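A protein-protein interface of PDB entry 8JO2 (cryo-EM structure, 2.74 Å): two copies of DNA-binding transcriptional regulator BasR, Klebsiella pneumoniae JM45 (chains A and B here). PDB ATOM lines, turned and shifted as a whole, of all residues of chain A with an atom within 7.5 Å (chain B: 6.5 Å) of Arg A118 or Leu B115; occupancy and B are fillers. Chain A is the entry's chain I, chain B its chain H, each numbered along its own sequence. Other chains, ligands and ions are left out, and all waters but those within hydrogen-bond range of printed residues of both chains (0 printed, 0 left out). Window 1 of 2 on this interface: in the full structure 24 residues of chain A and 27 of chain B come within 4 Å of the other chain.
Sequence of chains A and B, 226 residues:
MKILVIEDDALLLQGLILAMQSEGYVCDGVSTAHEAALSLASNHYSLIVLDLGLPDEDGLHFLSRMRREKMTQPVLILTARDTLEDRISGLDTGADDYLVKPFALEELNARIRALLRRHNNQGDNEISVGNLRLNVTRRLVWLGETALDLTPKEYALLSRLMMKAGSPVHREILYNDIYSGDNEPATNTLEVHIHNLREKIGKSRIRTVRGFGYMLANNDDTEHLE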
ATOM      1  N   PRO A  74     -36.467  12.371 -10.498  1.00  0.00           N
ATOM      2  CA  PRO A  74     -35.543  13.187  -9.707  1.00  0.00           C
ATOM      3  C   PRO A  74     -35.833  13.094  -8.222  1.00  0.00           C
ATOM      4  O   PRO A  74     -36.983  13.239  -7.802  1.00  0.00           O
ATOM      5  CB  PRO A  74     -35.803  14.600 -10.233  1.00  0.00           C
ATOM      6  CG  PRO A  74     -36.226  14.390 -11.636  1.00  0.00           C
ATOM      7  CD  PRO A  74     -37.007  13.107 -11.651  1.00  0.00           C
ATOM      8  N   LEU A  91     -25.199  10.189  -3.202  1.00  0.00           N
ATOM      9  CA  LEU A  91     -25.228  10.331  -4.654  1.00  0.00           C
ATOM     10  C   LEU A  91     -25.220   8.978  -5.350  1.00  0.00           C
ATOM     11  O   LEU A  91     -26.091   8.687  -6.177  1.00  0.00           O
ATOM     12  CB  LEU A  91     -24.046  11.176  -5.131  1.00  0.00           C
ATOM     13  CG  LEU A  91     -24.110  12.674  -4.854  1.00  0.00           C
ATOM     14  CD1 LEU A  91     -22.750  13.302  -5.082  1.00  0.00           C
ATOM     15  CD2 LEU A  91     -25.159  13.327  -5.736  1.00  0.00           C
ATOM     16  N   ALA A  95     -29.233   9.402  -5.147  1.00  0.00           N
ATOM     17  CA  ALA A  95     -29.567  10.809  -5.009  1.00  0.00           C
ATOM     18  C   ALA A  95     -29.023  11.607  -6.184  1.00  0.00           C
ATOM     19  O   ALA A  95     -27.939  11.321  -6.696  1.00  0.00           O
ATOM     20  CB  ALA A  95     -29.007  11.358  -3.702  1.00  0.00           C
ATOM     21  N   ASP A  96     -29.795  12.603  -6.622  1.00  0.00           N
ATOM     22  CA  ASP A  96     -29.374  13.425  -7.787  1.00  0.00           C
ATOM     23  C   ASP A  96     -28.662  14.686  -7.291  1.00  0.00           C
ATOM     24  O   ASP A  96     -27.505  14.890  -7.696  1.00  0.00           O
ATOM     25  CB  ASP A  96     -30.566  13.739  -8.692  1.00  0.00           C
ATOM     26  CG  ASP A  96     -31.233  12.493  -9.248  1.00  0.00           C
ATOM     27  OD1 ASP A  96     -30.754  11.986 -10.279  1.00  0.00           O
ATOM     28  OD2 ASP A  96     -32.220  12.036  -8.640  1.00  0.00           O
ATOM     29  N   ASP A  97     -29.315  15.488  -6.444  1.00  0.00           N
ATOM     30  CA  ASP A  97     -28.730  16.742  -5.989  1.00  0.00           C
ATOM     31  C   ASP A  97     -28.817  16.812  -4.472  1.00  0.00           C
ATOM     32  O   ASP A  97     -29.704  16.223  -3.855  1.00  0.00           O
ATOM     33  CB  ASP A  97     -29.417  17.967  -6.603  1.00  0.00           C
ATOM     34  CG  ASP A  97     -29.145  18.108  -8.086  1.00  0.00           C
ATOM     35  OD1 ASP A  97     -28.072  17.671  -8.539  1.00  0.00           O
ATOM     36  OD2 ASP A  97     -29.995  18.675  -8.798  1.00  0.00           O
ATOM     37  N   ALA A 110     -34.150  26.860  -7.698  1.00  0.00           N
ATOM     38  CA  ALA A 110     -33.323  26.755  -8.897  1.00  0.00           C
ATOM     39  C   ALA A 110     -32.921  25.311  -9.167  1.00  0.00           C
ATOM     40  O   ALA A 110     -33.030  24.823 -10.300  1.00  0.00           O
ATOM     41  CB  ALA A 110     -32.084  27.637  -8.758  1.00  0.00           C
ATOM     42  N   ARG A 111     -32.413  24.626  -8.140  1.00  0.00           N
ATOM     43  CA  ARG A 111     -32.083  23.212  -8.293  1.00  0.00           C
ATOM     44  C   ARG A 111     -33.292  22.438  -8.806  1.00  0.00           C
ATOM     45  O   ARG A 111     -33.178  21.590  -9.700  1.00  0.00           O
ATOM     46  CB  ARG A 111     -31.590  22.638  -6.964  1.00  0.00           C
ATOM     47  CG  ARG A 111     -30.385  23.356  -6.370  1.00  0.00           C
ATOM     48  CD  ARG A 111     -29.084  22.952  -7.040  1.00  0.00           C
ATOM     49  NE  ARG A 111     -27.922  23.616  -6.448  1.00  0.00           N
ATOM     50  CZ  ARG A 111     -26.659  23.386  -6.804  1.00  0.00           C
ATOM     51  NH1 ARG A 111     -25.670  24.038  -6.214  1.00  0.00           N
ATOM     52  NH2 ARG A 111     -26.382  22.511  -7.758  1.00  0.00           N
ATOM     53  N   ILE A 112     -34.452  22.705  -8.202  1.00  0.00           N
ATOM     54  CA  ILE A 112     -35.697  21.973  -8.579  1.00  0.00           C
ATOM     55  C   ILE A 112     -35.940  22.151 -10.082  1.00  0.00           C
ATOM     56  O   ILE A 112     -36.085  21.122 -10.787  1.00  0.00           O
ATOM     57  CB  ILE A 112     -36.874  22.473  -7.715  1.00  0.00           C
ATOM     58  CG1 ILE A 112     -36.793  21.938  -6.285  1.00  0.00           C
ATOM     59  CG2 ILE A 112     -38.209  22.132  -8.342  1.00  0.00           C
ATOM     60  CD1 ILE A 112     -38.068  22.111  -5.494  1.00  0.00           C
ATOM     61  N   ARG A 113     -35.947  23.400 -10.554  1.00  0.00           N
ATOM     62  CA  ARG A 113     -36.193  23.682 -11.990  1.00  0.00           C
ATOM     63  C   ARG A 113     -35.225  22.857 -12.834  1.00  0.00           C
ATOM     64  O   ARG A 113     -35.699  22.160 -13.754  1.00  0.00           O
ATOM     65  CB  ARG A 113     -35.991  25.171 -12.278  1.00  0.00           C
ATOM     66  CG  ARG A 113     -37.061  26.070 -11.678  1.00  0.00           C
ATOM     67  CD  ARG A 113     -36.834  27.532 -12.010  1.00  0.00           C
ATOM     68  NE  ARG A 113     -35.971  28.229 -11.066  1.00  0.00           N
ATOM     69  CZ  ARG A 113     -36.397  28.912 -10.007  1.00  0.00           C
ATOM     70  NH1 ARG A 113     -35.526  29.518  -9.219  1.00  0.00           N
ATOM     71  NH2 ARG A 113     -37.688  28.987  -9.737  1.00  0.00           N
ATOM     72  N   ALA A 114     -33.930  22.936 -12.520  1.00  0.00           N
ATOM     73  CA  ALA A 114     -32.905  22.197 -13.288  1.00  0.00           C
ATOM     74  C   ALA A 114     -33.294  20.719 -13.375  1.00  0.00           C
ATOM     75  O   ALA A 114     -33.435  20.225 -14.506  1.00  0.00           O
ATOM     76  CB  ALA A 114     -31.557  22.377 -12.640  1.00  0.00           C
ATOM     77  N   LEU A 115     -33.479  20.054 -12.232  1.00  0.00           N
ATOM     78  CA  LEU A 115     -33.806  18.603 -12.210  1.00  0.00           C
ATOM     79  C   LEU A 115     -35.020  18.311 -13.096  1.00  0.00           C
ATOM     80  O   LEU A 115     -34.956  17.342 -13.894  1.00  0.00           O
ATOM     81  CB  LEU A 115     -34.085  18.199 -10.762  1.00  0.00           C
ATOM     82  CG  LEU A 115     -32.909  17.564 -10.030  1.00  0.00           C
ATOM     83  CD1 LEU A 115     -33.324  17.068  -8.654  1.00  0.00           C
ATOM     84  CD2 LEU A 115     -32.307  16.436 -10.852  1.00  0.00           C
ATOM     85  N   LEU A 116     -36.087  19.102 -12.956  1.00  0.00           N
ATOM     86  CA  LEU A 116     -37.327  18.806 -13.724  1.00  0.00           C
ATOM     87  C   LEU A 116     -37.051  18.941 -15.223  1.00  0.00           C
ATOM     88  O   LEU A 116     -37.413  18.007 -15.976  1.00  0.00           O
ATOM     89  CB  LEU A 116     -38.423  19.765 -13.264  1.00  0.00           C
ATOM     90  CG  LEU A 116     -38.848  19.566 -11.812  1.00  0.00           C
ATOM     91  CD1 LEU A 116     -39.639  20.756 -11.304  1.00  0.00           C
ATOM     92  CD2 LEU A 116     -39.637  18.279 -11.654  1.00  0.00           C
ATOM     93  N   ARG A 117     -36.428  20.047 -15.630  1.00  0.00           N
ATOM     94  CA  ARG A 117     -36.123  20.269 -17.068  1.00  0.00           C
ATOM     95  C   ARG A 117     -35.240  19.119 -17.573  1.00  0.00           C
ATOM     96  O   ARG A 117     -35.348  18.779 -18.764  1.00  0.00           O
ATOM     97  CB  ARG A 117     -35.506  21.660 -17.260  1.00  0.00           C
ATOM     98  CG  ARG A 117     -36.435  22.834 -16.984  1.00  0.00           C
ATOM     99  CD  ARG A 117     -35.782  24.178 -17.238  1.00  0.00           C
ATOM    100  NE  ARG A 117     -36.649  25.301 -16.907  1.00  0.00           N
ATOM    101  CZ  ARG A 117     -36.283  26.578 -16.928  1.00  0.00           C
ATOM    102  NH1 ARG A 117     -37.156  27.519 -16.606  1.00  0.00           N
ATOM    103  NH2 ARG A 117     -35.052  26.915 -17.268  1.00  0.00           N
ATOM    104  N   ARG A 118     -34.402  18.544 -16.700  1.00  0.00           N
ATOM    105  CA  ARG A 118     -33.490  17.435 -17.096  1.00  0.00           C
ATOM    106  C   ARG A 118     -34.292  16.176 -17.420  1.00  0.00           C
ATOM    107  O   ARG A 118     -34.090  15.621 -18.515  1.00  0.00           O
ATOM    108  CB  ARG A 118     -32.519  17.101 -15.961  1.00  0.00           C
ATOM    109  CG  ARG A 118     -31.138  17.718 -16.114  1.00  0.00           C
ATOM    110  CD  ARG A 118     -30.284  17.411 -14.902  1.00  0.00           C
ATOM    111  NE  ARG A 118     -30.471  18.404 -13.854  1.00  0.00           N
ATOM    112  CZ  ARG A 118     -29.920  18.342 -12.648  1.00  0.00           C
ATOM    113  NH1 ARG A 118     -30.159  19.295 -11.765  1.00  0.00           N
ATOM    114  NH2 ARG A 118     -29.141  17.328 -12.321  1.00  0.00           N
ATOM    115  N   HIS A 119     -35.145  15.731 -16.493  1.00  0.00           N
ATOM    116  CA  HIS A 119     -35.912  14.471 -16.690  1.00  0.00           C
ATOM    117  C   HIS A 119     -36.949  14.667 -17.801  1.00  0.00           C
ATOM    118  O   HIS A 119     -37.329  13.656 -18.423  1.00  0.00           O
ATOM    119  CB  HIS A 119     -36.490  13.963 -15.359  1.00  0.00           C
ATOM    120  CG  HIS A 119     -37.914  14.322 -15.093  1.00  0.00           C
ATOM    121  ND1 HIS A 119     -38.272  15.490 -14.454  1.00  0.00           N
ATOM    122  CD2 HIS A 119     -39.063  13.654 -15.331  1.00  0.00           C
ATOM    123  CE1 HIS A 119     -39.581  15.540 -14.332  1.00  0.00           C
ATOM    124  NE2 HIS A 119     -40.091  14.425 -14.864  1.00  0.00           N
ATOM    125  N   ASN A 120     -37.379  15.909 -18.056  1.00  0.00           N
ATOM    126  CA  ASN A 120     -38.294  16.102 -19.215  1.00  0.00           C
ATOM    127  C   ASN A 120     -37.476  16.404 -20.479  1.00  0.00           C
ATOM    128  O   ASN A 120     -36.265  16.099 -20.486  1.00  0.00           O
ATOM    129  CB  ASN A 120     -39.333  17.193 -18.944  1.00  0.00           C
ATOM    130  CG  ASN A 120     -40.209  16.892 -17.747  1.00  0.00           C
ATOM    131  OD1 ASN A 120     -40.801  15.819 -17.663  1.00  0.00           O
ATOM    132  ND2 ASN A 120     -40.298  17.833 -16.822  1.00  0.00           N
ATOM    133  N   ASN A 121     -38.119  16.963 -21.512  1.00  0.00           N
ATOM    134  CA  ASN A 121     -37.427  17.326 -22.782  1.00  0.00           C
ATOM    135  C   ASN A 121     -36.586  16.143 -23.280  1.00  0.00           C
ATOM    136  O   ASN A 121     -35.393  16.351 -23.582  1.00  0.00           O
ATOM    137  CB  ASN A 121     -36.614  18.618 -22.638  1.00  0.00           C
ATOM    138  CG  ASN A 121     -37.289  19.657 -21.768  1.00  0.00           C
ATOM    139  OD1 ASN A 121     -38.480  19.923 -21.920  1.00  0.00           O
ATOM    140  ND2 ASN A 121     -36.540  20.245 -20.850  1.00  0.00           N
ATOM    141  N   GLN A 122     -37.189  14.953 -23.370  1.00  0.00           N
ATOM    142  CA  GLN A 122     -36.478  13.750 -23.879  1.00  0.00           C
ATOM    143  C   GLN A 122     -37.408  13.033 -24.863  1.00  0.00           C
ATOM    144  O   GLN A 122     -37.661  11.826 -24.669  1.00  0.00           O
ATOM    145  CB  GLN A 122     -36.059  12.858 -22.711  1.00  0.00           C
ATOM    146  CG  GLN A 122     -34.999  13.486 -21.819  1.00  0.00           C
ATOM    147  CD  GLN A 122     -34.670  12.603 -20.643  1.00  0.00           C
ATOM    148  OE1 GLN A 122     -35.479  11.785 -20.210  1.00  0.00           O
ATOM    149  NE2 GLN A 122     -33.467  12.761 -20.118  1.00  0.00           N
ATOM    150  N   LEU B  47     -20.552  14.750 -21.453  1.00  0.00           N
ATOM    151  CA  LEU B  47     -20.593  15.577 -20.263  1.00  0.00           C
ATOM    152  C   LEU B  47     -19.587  16.707 -20.420  1.00  0.00           C
ATOM    153  O   LEU B  47     -18.526  16.523 -21.020  1.00  0.00           O
ATOM    154  CB  LEU B  47     -20.264  14.766 -19.019  1.00  0.00           C
ATOM    155  CG  LEU B  47     -20.370  15.596 -17.751  1.00  0.00           C
ATOM    156  CD1 LEU B  47     -21.799  16.066 -17.565  1.00  0.00           C
ATOM    157  CD2 LEU B  47     -19.877  14.833 -16.560  1.00  0.00           C
ATOM    158  N   PRO B  74     -25.398  17.185 -20.316  1.00  0.00           N
ATOM    159  CA  PRO B  74     -25.334  17.816 -18.997  1.00  0.00           C
ATOM    160  C   PRO B  74     -24.050  18.608 -18.840  1.00  0.00           C
ATOM    161  O   PRO B  74     -23.021  18.290 -19.437  1.00  0.00           O
ATOM    162  CB  PRO B  74     -25.376  16.629 -18.027  1.00  0.00           C
ATOM    163  CG  PRO B  74     -25.125  15.421 -18.864  1.00  0.00           C
ATOM    164  CD  PRO B  74     -25.635  15.741 -20.219  1.00  0.00           C
ATOM    165  N   VAL B  75     -24.122  19.669 -18.046  1.00  0.00           N
ATOM    166  CA  VAL B  75     -22.968  20.511 -17.778  1.00  0.00           C
ATOM    167  C   VAL B  75     -22.812  20.641 -16.270  1.00  0.00           C
ATOM    168  O   VAL B  75     -23.760  21.014 -15.571  1.00  0.00           O
ATOM    169  CB  VAL B  75     -23.085  21.881 -18.456  1.00  0.00           C
ATOM    170  CG1 VAL B  75     -23.144  21.701 -19.962  1.00  0.00           C
ATOM    171  CG2 VAL B  75     -24.321  22.608 -17.989  1.00  0.00           C
ATOM    172  N   LEU B  76     -21.645  20.275 -15.765  1.00  0.00           N
ATOM    173  CA  LEU B  76     -21.308  20.435 -14.358  1.00  0.00           C
ATOM    174  C   LEU B  76     -20.319  21.587 -14.249  1.00  0.00           C
ATOM    175  O   LEU B  76     -19.243  21.546 -14.854  1.00  0.00           O
ATOM    176  CB  LEU B  76     -20.718  19.151 -13.792  1.00  0.00           C
ATOM    177  CG  LEU B  76     -19.985  19.341 -12.474  1.00  0.00           C
ATOM    178  CD1 LEU B  76     -20.982  19.718 -11.405  1.00  0.00           C
ATOM    179  CD2 LEU B  76     -19.236  18.083 -12.095  1.00  0.00           C
ATOM    180  N   ALA B  95     -26.895  25.293 -16.240  1.00  0.00           N
ATOM    181  CA  ALA B  95     -25.984  24.478 -15.445  1.00  0.00           C
ATOM    182  C   ALA B  95     -26.794  23.435 -14.686  1.00  0.00           C
ATOM    183  O   ALA B  95     -27.636  23.783 -13.854  1.00  0.00           O
ATOM    184  CB  ALA B  95     -25.184  25.353 -14.485  1.00  0.00           C
ATOM    185  N   ASP B  96     -26.565  22.154 -14.981  1.00  0.00           N
ATOM    186  CA  ASP B  96     -27.340  21.102 -14.328  1.00  0.00           C
ATOM    187  C   ASP B  96     -26.908  20.895 -12.884  1.00  0.00           C
ATOM    188  O   ASP B  96     -27.749  20.724 -11.996  1.00  0.00           O
ATOM    189  CB  ASP B  96     -27.224  19.804 -15.111  1.00  0.00           C
ATOM    190  CG  ASP B  96     -27.919  19.886 -16.432  1.00  0.00           C
ATOM    191  OD1 ASP B  96     -28.898  20.654 -16.519  1.00  0.00           O
ATOM    192  OD2 ASP B  96     -27.506  19.182 -17.369  1.00  0.00           O
ATOM    193  N   ASP B  97     -25.607  20.884 -12.633  1.00  0.00           N
ATOM    194  CA  ASP B  97     -25.096  20.832 -11.277  1.00  0.00           C
ATOM    195  C   ASP B  97     -23.929  21.795 -11.180  1.00  0.00           C
ATOM    196  O   ASP B  97     -23.216  22.037 -12.155  1.00  0.00           O
ATOM    197  CB  ASP B  97     -24.664  19.421 -10.873  1.00  0.00           C
ATOM    198  CG  ASP B  97     -24.892  19.150  -9.401  1.00  0.00           C
ATOM    199  OD1 ASP B  97     -24.604  20.051  -8.588  1.00  0.00           O
ATOM    200  OD2 ASP B  97     -25.343  18.040  -9.054  1.00  0.00           O
ATOM    201  N   ALA B 110     -18.405  11.663  -8.021  1.00  0.00           N
ATOM    202  CA  ALA B 110     -19.745  11.220  -7.652  1.00  0.00           C
ATOM    203  C   ALA B 110     -20.812  12.065  -8.332  1.00  0.00           C
ATOM    204  O   ALA B 110     -21.811  11.536  -8.836  1.00  0.00           O
ATOM    205  CB  ALA B 110     -19.910  11.265  -6.135  1.00  0.00           C
ATOM    206  N   ARG B 111     -20.628  13.383  -8.337  1.00  0.00           N
ATOM    207  CA  ARG B 111     -21.577  14.255  -9.018  1.00  0.00           C
ATOM    208  C   ARG B 111     -21.695  13.877 -10.489  1.00  0.00           C
ATOM    209  O   ARG B 111     -22.801  13.763 -11.035  1.00  0.00           O
ATOM    210  CB  ARG B 111     -21.135  15.707  -8.866  1.00  0.00           C
ATOM    211  CG  ARG B 111     -21.463  16.316  -7.520  1.00  0.00           C
ATOM    212  CD  ARG B 111     -22.884  16.818  -7.473  1.00  0.00           C
ATOM    213  NE  ARG B 111     -23.105  17.678  -6.318  1.00  0.00           N
ATOM    214  CZ  ARG B 111     -24.294  17.903  -5.776  1.00  0.00           C
ATOM    215  NH1 ARG B 111     -25.374  17.333  -6.288  1.00  0.00           N
ATOM    216  NH2 ARG B 111     -24.404  18.701  -4.727  1.00  0.00           N
ATOM    217  N   ILE B 112     -20.553  13.675 -11.143  1.00  0.00           N
ATOM    218  CA  ILE B 112     -20.552  13.281 -12.547  1.00  0.00           C
ATOM    219  C   ILE B 112     -21.295  11.968 -12.740  1.00  0.00           C
ATOM    220  O   ILE B 112     -22.100  11.822 -13.666  1.00  0.00           O
ATOM    221  CB  ILE B 112     -19.110  13.200 -13.072  1.00  0.00           C
ATOM    222  CG1 ILE B 112     -18.538  14.602 -13.239  1.00  0.00           C
ATOM    223  CG2 ILE B 112     -19.020  12.365 -14.328  1.00  0.00           C
ATOM    224  CD1 ILE B 112     -17.137  14.605 -13.696  1.00  0.00           C
ATOM    225  N   ARG B 113     -20.997  10.978 -11.901  1.00  0.00           N
ATOM    226  CA  ARG B 113     -21.657   9.684 -12.012  1.00  0.00           C
ATOM    227  C   ARG B 113     -23.168   9.848 -11.946  1.00  0.00           C
ATOM    228  O   ARG B 113     -23.908   9.286 -12.762  1.00  0.00           O
ATOM    229  CB  ARG B 113     -21.162   8.746 -10.912  1.00  0.00           C
ATOM    230  CG  ARG B 113     -21.093   7.295 -11.343  1.00  0.00           C
ATOM    231  CD  ARG B 113     -19.839   6.596 -10.846  1.00  0.00           C
ATOM    232  NE  ARG B 113     -19.704   6.666  -9.396  1.00  0.00           N
ATOM    233  CZ  ARG B 113     -18.677   7.221  -8.767  1.00  0.00           C
ATOM    234  NH1 ARG B 113     -17.676   7.742  -9.459  1.00  0.00           N
ATOM    235  NH2 ARG B 113     -18.644   7.239  -7.442  1.00  0.00           N
ATOM    236  N   ALA B 114     -23.640  10.619 -10.968  1.00  0.00           N
ATOM    237  CA  ALA B 114     -25.068  10.881 -10.850  1.00  0.00           C
ATOM    238  C   ALA B 114     -25.621  11.504 -12.123  1.00  0.00           C
ATOM    239  O   ALA B 114     -26.684  11.107 -12.613  1.00  0.00           O
ATOM    240  CB  ALA B 114     -25.336  11.785  -9.649  1.00  0.00           C
ATOM    241  N   LEU B 115     -24.919  12.502 -12.661  1.00  0.00           N
ATOM    242  CA  LEU B 115     -25.411  13.181 -13.859  1.00  0.00           C
ATOM    243  C   LEU B 115     -25.554  12.224 -15.036  1.00  0.00           C
ATOM    244  O   LEU B 115     -26.596  12.194 -15.701  1.00  0.00           O
ATOM    245  CB  LEU B 115     -24.492  14.343 -14.225  1.00  0.00           C
ATOM    246  CG  LEU B 115     -24.586  15.522 -13.269  1.00  0.00           C
ATOM    247  CD1 LEU B 115     -23.759  16.672 -13.790  1.00  0.00           C
ATOM    248  CD2 LEU B 115     -26.031  15.930 -13.104  1.00  0.00           C
ATOM    249  N   LEU B 116     -24.437  11.577 -15.375  1.00  0.00           N
ATOM    250  CA  LEU B 116     -24.380  10.574 -16.466  1.00  0.00           C
ATOM    251  C   LEU B 116     -25.546   9.605 -16.346  1.00  0.00           C
ATOM    252  O   LEU B 116     -26.224   9.367 -17.360  1.00  0.00           O
ATOM    253  CB  LEU B 116     -23.089   9.834 -16.131  1.00  0.00           C
ATOM    254  CG  LEU B 116     -22.364   9.086 -17.234  1.00  0.00           C
ATOM    255  CD1 LEU B 116     -21.119   9.859 -17.645  1.00  0.00           C
ATOM    256  CD2 LEU B 116     -21.980   7.707 -16.720  1.00  0.00           C
ATOM    257  N   ARG B 117     -25.768   9.077 -15.147  1.00  0.00           N
ATOM    258  CA  ARG B 117     -26.813   8.058 -14.880  1.00  0.00           C
ATOM    259  C   ARG B 117     -28.191   8.650 -15.196  1.00  0.00           C
ATOM    260  O   ARG B 117     -28.917   8.031 -15.986  1.00  0.00           O
ATOM    261  CB  ARG B 117     -26.694   7.580 -13.430  1.00  0.00           C
ATOM    262  CG  ARG B 117     -27.913   6.848 -12.890  1.00  0.00           C
ATOM    263  CD  ARG B 117     -27.902   6.768 -11.376  1.00  0.00           C
ATOM    264  NE  ARG B 117     -28.496   7.948 -10.767  1.00  0.00           N
ATOM    265  CZ  ARG B 117     -28.034   8.557  -9.680  1.00  0.00           C
ATOM    266  NH1 ARG B 117     -28.651   9.628  -9.214  1.00  0.00           N
ATOM    267  NH2 ARG B 117     -26.960   8.096  -9.064  1.00  0.00           N
ATOM    268  N   ARG B 118     -28.528   9.818 -14.636  1.00  0.00           N
ATOM    269  CA  ARG B 118     -29.885  10.407 -14.825  1.00  0.00           C
ATOM    270  C   ARG B 118     -30.140  10.655 -16.316  1.00  0.00           C
ATOM    271  O   ARG B 118     -31.265  10.375 -16.770  1.00  0.00           O
ATOM    272  CB  ARG B 118     -30.033  11.678 -13.979  1.00  0.00           C
ATOM    273  CG  ARG B 118     -31.127  12.640 -14.421  1.00  0.00           C
ATOM    274  CD  ARG B 118     -32.526  12.276 -13.958  1.00  0.00           C
ATOM    275  NE  ARG B 118     -32.561  11.648 -12.646  1.00  0.00           N
ATOM    276  CZ  ARG B 118     -33.496  10.795 -12.245  1.00  0.00           C
ATOM    277  NH1 ARG B 118     -34.483  10.462 -13.058  1.00  0.00           N
ATOM    278  NH2 ARG B 118     -33.437  10.275 -11.032  1.00  0.00           N
ATOM    279  N   HIS B 119     -29.131  11.125 -17.050  1.00  0.00           N
ATOM    280  CA  HIS B 119     -29.339  11.479 -18.479  1.00  0.00           C
ATOM    281  C   HIS B 119     -29.378  10.226 -19.353  1.00  0.00           C
ATOM    282  O   HIS B 119     -30.443   9.963 -19.939  1.00  0.00           O
ATOM    283  CB  HIS B 119     -28.251  12.461 -18.938  1.00  0.00           C
ATOM    284  CG  HIS B 119     -28.248  12.733 -20.404  1.00  0.00           C
ATOM    285  ND1 HIS B 119     -29.382  13.127 -21.086  1.00  0.00           N
ATOM    286  CD2 HIS B 119     -27.257  12.675 -21.318  1.00  0.00           C
ATOM    287  CE1 HIS B 119     -29.089  13.298 -22.358  1.00  0.00           C
ATOM    288  NE2 HIS B 119     -27.791  13.027 -22.526  1.00  0.00           N
ATOM    289  N   ASN B 120     -28.278   9.476 -19.425  1.00  0.00           N
ATOM    290  CA  ASN B 120     -28.209   8.328 -20.370  1.00  0.00           C
ATOM    291  C   ASN B 120     -28.970   7.106 -19.839  1.00  0.00           C
ATOM    292  O   ASN B 120     -29.820   6.591 -20.588  1.00  0.00           O
ATOM    293  CB  ASN B 120     -26.757   8.013 -20.727  1.00  0.00           C
ATOM    294  CG  ASN B 120     -25.980   9.246 -21.134  1.00  0.00           C
ATOM    295  OD1 ASN B 120     -25.391   9.918 -20.293  1.00  0.00           O
ATOM    296  ND2 ASN B 120     -25.975   9.549 -22.421  1.00  0.00           N
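The backbone NH of Asp B96 is in hydrogen-bond range of the backbone carbonyl oxygen of Val B75, at 3.1 Å.
The backbone carbonyl oxygen of Val B75 sits at hydrogen-bond distance from the backbone NH of Asp B97.
The side-chain carboxylate (OD2) of Asp B97 lies within salt-bridge range of the guanidinium group (NH1) of Arg B111, 2.9 Å away.
The side-chain carboxylate (OD2) of Asp A97 is in salt-bridge range of the guanidinium group (NH1) of Arg A118, 3.0 Å away.
The side-chain amide nitrogen (NE2) of Gln A122 is in hydrogen-bond range of the backbone carbonyl oxygen (O) of Arg A118.
Of the 18 printed residues of chain A, 7 touch a printed residue of chain B.
Hydrophobic or aromatic side chains of chain A within 4 Å of the printed part of chain B: Pro A74 and Leu A91.
Of the 18 printed residues of chain B, 8 touch a printed residue of chain A.
Among the printed residues, merely in contact across the chains: Pro A74 with Arg B118 (3.7 Å), Leu A91 with Ala B110 (3.7 Å), Leu A91 with Arg B111 (3.9 Å), Ala A95 with Ala B114 (3.96 Å), Asp A96 with Arg B111 (3.5 Å) and Arg A118 with Leu B115 (3.5 Å).
Printed residues of chain B within 4 Å of Leu A91: Ala B110 (3.7 Å), Arg B111 (3.9 Å) and Arg B117 (3.1 Å).
Arg A118 touches just these residues of chain B: Asp B96 and Leu B115.
His A119 touches none of the printed residues of chain B.
Of the printed residues of chain A, Ala B110 touches Leu A91.
Of chain A, only Ala A95 comes within 4 Å of Ala B114.
Of chain A, only Arg A118 comes within 4 Å of Leu B115.
The nearest residue of chain B that does not touch Arg A118 is Arg B118 (4.9 Å).
The nearest residue of chain A that does not touch Leu B115 is Asp A97 (5.3 Å).
The nearest printed residue of chain A that does not touch Arg B111 is Arg A111 (5.3 Å).
Asp A96 touches Arg B117, but with the chains exchanged Arg A117 does not touch Asp B96 (6.6 Å).
Asp A97 touches its own counterpart, Asp B97.
Asp A97 touches Arg B111, and with the chains exchanged Arg A111 touches Asp B97.
Arg A118 touches Leu B115, but with the chains exchanged Leu A115 does not touch Arg B118 (5.1 Å).
15 positions are printed for both chains.
Of the 14 pairs that touch across the chains among the printed residues, 5 have their exchanged pair printed and touching as well.
The guanidinium group (NE) of Arg A118 lies within salt-bridge range of the side-chain carboxylate (OD1) of Asp B96 (3.8 Å).
The guanidinium group (NH2) of Arg A111 is in salt-bridge range of the side-chain carboxylate (OD1) of Asp B97 (3.1 Å).
The side-chain carboxylate of Asp A97 is in salt-bridge range of the guanidinium group of Arg B111 (3.5 Å).
The guanidinium group (NH2) of Arg B117 lies within hydrogen-bond range of the backbone carbonyl oxygen (O) of Leu A91.
NH1 of Arg B117 is in hydrogen-bond range of O of Ala A95, 3.1 Å away.
The side-chain carboxylate (OD1) of Asp A96 lies within salt-bridge range of the guanidinium group (NH1) of Arg B117, 3.3 Å away.
The guanidinium group (NE) of Arg B118 lies within salt-bridge range of the side-chain carboxylate (OD1) of Asp A96 (3.0 Å).
OD2 of Asp B97 lies close to OD1 of Asp A97.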
